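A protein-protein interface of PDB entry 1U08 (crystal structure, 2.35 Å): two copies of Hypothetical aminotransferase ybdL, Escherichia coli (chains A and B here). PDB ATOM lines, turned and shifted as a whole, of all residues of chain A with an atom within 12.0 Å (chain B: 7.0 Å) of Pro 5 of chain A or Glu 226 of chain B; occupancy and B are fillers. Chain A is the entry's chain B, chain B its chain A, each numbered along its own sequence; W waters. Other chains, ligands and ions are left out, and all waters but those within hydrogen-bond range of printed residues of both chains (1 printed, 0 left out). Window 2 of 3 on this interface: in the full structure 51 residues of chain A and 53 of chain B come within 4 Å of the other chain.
No position is printed for both chains.
Water W1 lies within hydrogen-bond range of O of Glu 226 of chain B (2.6 Å) and O of Leu 6 of chain A (2.8 Å).
Of chain B, only Glu 226 (2.8 Å) comes within 4 Å of Pro 5 of chain A.
Of the printed residues of chain B, Leu 6 of chain A touches Phe 198 (3.5 Å), Glu 226 (3.97 Å) and Arg 227 (3.6 Å).
Of the printed residues of chain B, Pro 8 of chain A touches Phe 198, Pro 253 and Ile 254.
Val 218 of chain B touches none of the printed residues of chain A.
No residue of chain A comes within 4 Å of Arg 225 of chain B.
Of chain A, only Pro 5 (2.8 Å) and Leu 6 (3.97 Å) come within 4 Å of Glu 226 of chain B.
Of the printed residues of chain A, Arg 227 of chain B touches Leu 6 (3.6 Å).
No residue of chain A comes within 4 Å of Ala 228 of chain B.
No residue of chain A comes within 4 Å of Pro 251 of chain B.
The nearest residue of chain B that does not touch Pro 5 of chain A is Arg 227 of chain B (6.2 Å).
The nearest residue of chain A that does not touch Glu 226 of chain B is Ile 7 of chain A (6.2 Å).
Of the 5 printed residues of chain A, 4 touch a printed residue of chain B.
Hydrophobic or aromatic side chains of chain A that line the printed part of chain B: Pro 5, Leu 6 and Pro 8.
Along chain A the printed residues that touch a printed residue of chain B span positions 5 to 8.
Hydrophobic or aromatic side chains of chain B that line the printed part of chain A: Phe 198 and Ile 254.
Among the printed residues, 8 pairs touch across the chains.
OE1 of Glu 226 of chain B touches CG of Pro 5 of chain A, at 2.8 Å.
Phe 198 of chain B touches Leu 6 of chain A.
Glu 226 of chain B touches Leu 6 of chain A.
Leu 6 of chain A touches Arg 227 of chain B (CD2 to NE, 3.6 Å).
Phe 198 of chain B touches Ile 7 of chain A (CZ to C, 3.98 Å).
CG of Pro 8 of chain A touches CZ of Phe 198 of chain B, at 3.6 Å.
Pro 8 of chain A touches Pro 253 of chain B (CD to O, 3.9 Å).
Pro 8 of chain A touches Ile 254 of chain B.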
ATOM      1  N   PRO A   5      24.283   7.823 -26.727  1.00  0.00           N
ATOM      2  CA  PRO A   5      23.183   8.290 -27.571  1.00  0.00           C
ATOM      3  C   PRO A   5      23.400   8.512 -29.057  1.00  0.00           C
ATOM      4  O   PRO A   5      24.007   9.490 -29.502  1.00  0.00           O
ATOM      5  CB  PRO A   5      22.602   9.464 -26.862  1.00  0.00           C
ATOM      6  CG  PRO A   5      22.776   9.077 -25.381  1.00  0.00           C
ATOM      7  CD  PRO A   5      24.127   8.227 -25.307  1.00  0.00           C
ATOM      8  N   LEU A   6      22.852   7.551 -29.790  1.00  0.00           N
ATOM      9  CA  LEU A   6      22.909   7.496 -31.226  1.00  0.00           C
ATOM     10  C   LEU A   6      21.793   8.356 -31.840  1.00  0.00           C
ATOM     11  O   LEU A   6      20.614   8.180 -31.524  1.00  0.00           O
ATOM     12  CB  LEU A   6      22.747   6.038 -31.559  1.00  0.00           C
ATOM     13  CG  LEU A   6      22.692   5.402 -32.927  1.00  0.00           C
ATOM     14  CD1 LEU A   6      23.974   5.627 -33.684  1.00  0.00           C
ATOM     15  CD2 LEU A   6      22.457   3.920 -32.713  1.00  0.00           C
ATOM     16  N   ILE A   7      22.176   9.268 -32.730  1.00  0.00           N
ATOM     17  CA  ILE A   7      21.227  10.167 -33.385  1.00  0.00           C
ATOM     18  C   ILE A   7      20.941   9.860 -34.869  1.00  0.00           C
ATOM     19  O   ILE A   7      21.850   9.829 -35.700  1.00  0.00           O
ATOM     20  CB  ILE A   7      21.708  11.643 -33.273  1.00  0.00           C
ATOM     21  CG1 ILE A   7      21.886  12.010 -31.799  1.00  0.00           C
ATOM     22  CG2 ILE A   7      20.681  12.591 -33.911  1.00  0.00           C
ATOM     23  CD1 ILE A   7      23.077  12.899 -31.522  1.00  0.00           C
ATOM     24  N   PRO A   8      19.656   9.661 -35.222  1.00  0.00           N
ATOM     25  CA  PRO A   8      19.273   9.364 -36.610  1.00  0.00           C
ATOM     26  C   PRO A   8      19.439  10.565 -37.539  1.00  0.00           C
ATOM     27  O   PRO A   8      19.247  11.713 -37.126  1.00  0.00           O
ATOM     28  CB  PRO A   8      17.795   8.968 -36.503  1.00  0.00           C
ATOM     29  CG  PRO A   8      17.568   8.732 -35.037  1.00  0.00           C
ATOM     30  CD  PRO A   8      18.460   9.729 -34.371  1.00  0.00           C
ATOM     31  N   GLN A   9      19.791  10.293 -38.792  1.00  0.00           N
ATOM     32  CA  GLN A   9      19.954  11.338 -39.801  1.00  0.00           C
ATOM     33  C   GLN A   9      18.622  11.468 -40.529  1.00  0.00           C
ATOM     34  O   GLN A   9      18.269  10.616 -41.344  1.00  0.00           O
ATOM     35  CB  GLN A   9      21.053  10.951 -40.790  1.00  0.00           C
ATOM     36  CG  GLN A   9      22.464  11.214 -40.278  1.00  0.00           C
ATOM     37  CD  GLN A   9      23.501  10.276 -40.882  1.00  0.00           C
ATOM     38  OE1 GLN A   9      23.478   9.989 -42.082  1.00  0.00           O
ATOM     39  NE2 GLN A   9      24.426   9.805 -40.050  1.00  0.00           N
ATOM     40  N   TRP B 189      23.005  -6.216 -26.968  1.00  0.00           N
ATOM     41  CA  TRP B 189      23.810  -5.022 -26.761  1.00  0.00           C
ATOM     42  C   TRP B 189      25.280  -5.317 -27.061  1.00  0.00           C
ATOM     43  O   TRP B 189      25.936  -4.547 -27.757  1.00  0.00           O
ATOM     44  CB  TRP B 189      23.667  -4.514 -25.323  1.00  0.00           C
ATOM     45  CG  TRP B 189      24.618  -3.404 -25.001  1.00  0.00           C
ATOM     46  CD1 TRP B 189      25.632  -3.430 -24.085  1.00  0.00           C
ATOM     47  CD2 TRP B 189      24.659  -2.107 -25.605  1.00  0.00           C
ATOM     48  NE1 TRP B 189      26.304  -2.231 -24.083  1.00  0.00           N
ATOM     49  CE2 TRP B 189      25.727  -1.400 -25.007  1.00  0.00           C
ATOM     50  CE3 TRP B 189      23.897  -1.472 -26.595  1.00  0.00           C
ATOM     51  CZ2 TRP B 189      26.051  -0.087 -25.365  1.00  0.00           C
ATOM     52  CZ3 TRP B 189      24.219  -0.167 -26.951  1.00  0.00           C
ATOM     53  CH2 TRP B 189      25.287   0.511 -26.336  1.00  0.00           C
ATOM     54  N   PHE B 198      20.288   0.687 -34.921  1.00  0.00           N
ATOM     55  CA  PHE B 198      19.129   1.028 -34.122  1.00  0.00           C
ATOM     56  C   PHE B 198      18.336  -0.251 -33.898  1.00  0.00           C
ATOM     57  O   PHE B 198      18.507  -1.230 -34.623  1.00  0.00           O
ATOM     58  CB  PHE B 198      18.269   2.057 -34.858  1.00  0.00           C
ATOM     59  CG  PHE B 198      18.874   3.435 -34.906  1.00  0.00           C
ATOM     60  CD1 PHE B 198      18.815   4.272 -33.805  1.00  0.00           C
ATOM     61  CD2 PHE B 198      19.491   3.896 -36.062  1.00  0.00           C
ATOM     62  CE1 PHE B 198      19.357   5.553 -33.851  1.00  0.00           C
ATOM     63  CE2 PHE B 198      20.036   5.174 -36.115  1.00  0.00           C
ATOM     64  CZ  PHE B 198      19.966   6.003 -35.005  1.00  0.00           C
ATOM     65  N   VAL B 218      12.957  -3.984 -23.947  1.00  0.00           N
ATOM     66  CA  VAL B 218      14.166  -3.333 -24.422  1.00  0.00           C
ATOM     67  C   VAL B 218      14.341  -2.053 -23.605  1.00  0.00           C
ATOM     68  O   VAL B 218      15.452  -1.559 -23.435  1.00  0.00           O
ATOM     69  CB  VAL B 218      14.060  -2.985 -25.925  1.00  0.00           C
ATOM     70  CG1 VAL B 218      12.981  -1.930 -26.152  1.00  0.00           C
ATOM     71  CG2 VAL B 218      15.404  -2.501 -26.429  1.00  0.00           C
ATOM     72  N   HIS B 221      16.719  -2.063 -20.518  1.00  0.00           N
ATOM     73  CA  HIS B 221      18.163  -2.085 -20.720  1.00  0.00           C
ATOM     74  C   HIS B 221      18.646  -0.656 -20.934  1.00  0.00           C
ATOM     75  O   HIS B 221      18.375  -0.042 -21.963  1.00  0.00           O
ATOM     76  CB  HIS B 221      18.523  -2.962 -21.922  1.00  0.00           C
ATOM     77  CG  HIS B 221      19.983  -3.286 -22.011  1.00  0.00           C
ATOM     78  ND1 HIS B 221      20.932  -2.354 -22.371  1.00  0.00           N
ATOM     79  CD2 HIS B 221      20.659  -4.430 -21.748  1.00  0.00           C
ATOM     80  CE1 HIS B 221      22.130  -2.910 -22.327  1.00  0.00           C
ATOM     81  NE2 HIS B 221      21.992  -4.170 -21.952  1.00  0.00           N
ATOM     82  N   PRO B 222      19.386  -0.116 -19.957  1.00  0.00           N
ATOM     83  CA  PRO B 222      19.932   1.247 -19.972  1.00  0.00           C
ATOM     84  C   PRO B 222      20.591   1.704 -21.274  1.00  0.00           C
ATOM     85  O   PRO B 222      20.389   2.837 -21.709  1.00  0.00           O
ATOM     86  CB  PRO B 222      20.917   1.238 -18.804  1.00  0.00           C
ATOM     87  CG  PRO B 222      20.327   0.217 -17.866  1.00  0.00           C
ATOM     88  CD  PRO B 222      19.917  -0.876 -18.811  1.00  0.00           C
ATOM     89  N   GLN B 223      21.374   0.829 -21.896  1.00  0.00           N
ATOM     90  CA  GLN B 223      22.066   1.193 -23.121  1.00  0.00           C
ATOM     91  C   GLN B 223      21.261   0.995 -24.404  1.00  0.00           C
ATOM     92  O   GLN B 223      21.221   1.887 -25.252  1.00  0.00           O
ATOM     93  CB  GLN B 223      23.401   0.442 -23.209  1.00  0.00           C
ATOM     94  CG  GLN B 223      24.456   0.920 -22.201  1.00  0.00           C
ATOM     95  CD  GLN B 223      24.763  -0.112 -21.127  1.00  0.00           C
ATOM     96  OE1 GLN B 223      23.949  -0.377 -20.245  1.00  0.00           O
ATOM     97  NE2 GLN B 223      25.947  -0.710 -21.210  1.00  0.00           N
ATOM     98  N   LEU B 224      20.629  -0.164 -24.556  1.00  0.00           N
ATOM     99  CA  LEU B 224      19.833  -0.439 -25.749  1.00  0.00           C
ATOM    100  C   LEU B 224      18.737   0.607 -25.885  1.00  0.00           C
ATOM    101  O   LEU B 224      18.370   1.017 -26.985  1.00  0.00           O
ATOM    102  CB  LEU B 224      19.201  -1.825 -25.659  1.00  0.00           C
ATOM    103  CG  LEU B 224      20.074  -2.998 -26.089  1.00  0.00           C
ATOM    104  CD1 LEU B 224      19.352  -4.306 -25.818  1.00  0.00           C
ATOM    105  CD2 LEU B 224      20.403  -2.859 -27.568  1.00  0.00           C
ATOM    106  N   ARG B 225      18.232   1.031 -24.737  1.00  0.00           N
ATOM    107  CA  ARG B 225      17.175   2.024 -24.625  1.00  0.00           C
ATOM    108  C   ARG B 225      17.403   3.329 -25.399  1.00  0.00           C
ATOM    109  O   ARG B 225      16.513   3.781 -26.125  1.00  0.00           O
ATOM    110  CB  ARG B 225      16.965   2.336 -23.143  1.00  0.00           C
ATOM    111  CG  ARG B 225      16.123   3.546 -22.855  1.00  0.00           C
ATOM    112  CD  ARG B 225      16.329   3.961 -21.419  1.00  0.00           C
ATOM    113  NE  ARG B 225      16.015   2.867 -20.512  1.00  0.00           N
ATOM    114  CZ  ARG B 225      16.425   2.806 -19.251  1.00  0.00           C
ATOM    115  NH1 ARG B 225      17.173   3.777 -18.746  1.00  0.00           N
ATOM    116  NH2 ARG B 225      16.077   1.774 -18.491  1.00  0.00           N
ATOM    117  N   GLU B 226      18.580   3.936 -25.247  1.00  0.00           N
ATOM    118  CA  GLU B 226      18.860   5.193 -25.929  1.00  0.00           C
ATOM    119  C   GLU B 226      19.147   5.060 -27.422  1.00  0.00           C
ATOM    120  O   GLU B 226      19.625   6.003 -28.061  1.00  0.00           O
ATOM    121  CB  GLU B 226      19.991   5.953 -25.231  1.00  0.00           C
ATOM    122  CG  GLU B 226      21.259   5.170 -24.977  1.00  0.00           C
ATOM    123  CD  GLU B 226      22.290   5.988 -24.210  1.00  0.00           C
ATOM    124  OE1 GLU B 226      21.919   7.057 -23.672  1.00  0.00           O
ATOM    125  OE2 GLU B 226      23.468   5.562 -24.137  1.00  0.00           O
ATOM    126  N   ARG B 227      18.842   3.890 -27.980  1.00  0.00           N
ATOM    127  CA  ARG B 227      19.019   3.663 -29.413  1.00  0.00           C
ATOM    128  C   ARG B 227      17.917   2.726 -29.924  1.00  0.00           C
ATOM    129  O   ARG B 227      18.004   2.173 -31.028  1.00  0.00           O
ATOM    130  CB  ARG B 227      20.393   3.056 -29.717  1.00  0.00           C
ATOM    131  CG  ARG B 227      20.553   1.608 -29.299  1.00  0.00           C
ATOM    132  CD  ARG B 227      21.647   0.947 -30.112  1.00  0.00           C
ATOM    133  NE  ARG B 227      22.920   1.653 -29.990  1.00  0.00           N
ATOM    134  CZ  ARG B 227      24.053   1.238 -30.545  1.00  0.00           C
ATOM    135  NH1 ARG B 227      24.065   0.124 -31.263  1.00  0.00           N
ATOM    136  NH2 ARG B 227      25.172   1.926 -30.366  1.00  0.00           N
ATOM    137  N   ALA B 228      16.865   2.568 -29.127  1.00  0.00           N
ATOM    138  CA  ALA B 228      15.788   1.676 -29.518  1.00  0.00           C
ATOM    139  C   ALA B 228      14.384   2.272 -29.531  1.00  0.00           C
ATOM    140  O   ALA B 228      14.130   3.351 -28.989  1.00  0.00           O
ATOM    141  CB  ALA B 228      15.811   0.448 -28.624  1.00  0.00           C
ATOM    142  N   ALA B 250      10.718   6.081 -27.576  1.00  0.00           N
ATOM    143  CA  ALA B 250      12.075   6.220 -28.075  1.00  0.00           C
ATOM    144  C   ALA B 250      12.682   7.534 -27.617  1.00  0.00           C
ATOM    145  O   ALA B 250      11.965   8.451 -27.208  1.00  0.00           O
ATOM    146  CB  ALA B 250      12.081   6.146 -29.596  1.00  0.00           C
ATOM    147  N   PRO B 251      14.024   7.635 -27.667  1.00  0.00           N
ATOM    148  CA  PRO B 251      14.737   8.851 -27.256  1.00  0.00           C
ATOM    149  C   PRO B 251      14.266  10.026 -28.111  1.00  0.00           C
ATOM    150  O   PRO B 251      13.927   9.844 -29.280  1.00  0.00           O
ATOM    151  CB  PRO B 251      16.202   8.501 -27.511  1.00  0.00           C
ATOM    152  CG  PRO B 251      16.238   7.004 -27.340  1.00  0.00           C
ATOM    153  CD  PRO B 251      14.970   6.566 -28.043  1.00  0.00           C
ATOM    154  N   PRO B 253      15.533  12.263 -29.965  1.00  0.00           N
ATOM    155  CA  PRO B 253      16.045  12.336 -31.338  1.00  0.00           C
ATOM    156  C   PRO B 253      15.405  11.332 -32.292  1.00  0.00           C
ATOM    157  O   PRO B 253      15.149  11.646 -33.458  1.00  0.00           O
ATOM    158  CB  PRO B 253      17.539  12.079 -31.163  1.00  0.00           C
ATOM    159  CG  PRO B 253      17.817  12.606 -29.791  1.00  0.00           C
ATOM    160  CD  PRO B 253      16.642  12.082 -29.008  1.00  0.00           C
ATOM    161  N   ILE B 254      15.155  10.123 -31.805  1.00  0.00           N
ATOM    162  CA  ILE B 254      14.554   9.090 -32.640  1.00  0.00           C
ATOM    163  C   ILE B 254      13.058   9.336 -32.771  1.00  0.00           C
ATOM    164  O   ILE B 254      12.476   9.154 -33.846  1.00  0.00           O
ATOM    165  CB  ILE B 254      14.808   7.682 -32.056  1.00  0.00           C
ATOM    166  CG1 ILE B 254      16.319   7.413 -32.010  1.00  0.00           C
ATOM    167  CG2 ILE B 254      14.114   6.624 -32.918  1.00  0.00           C
ATOM    168  CD1 ILE B 254      16.702   6.133 -31.313  1.00  0.00           C
HETATM  169  O   HOH W   1      19.009   8.291 -29.204  1.00  0.00           O
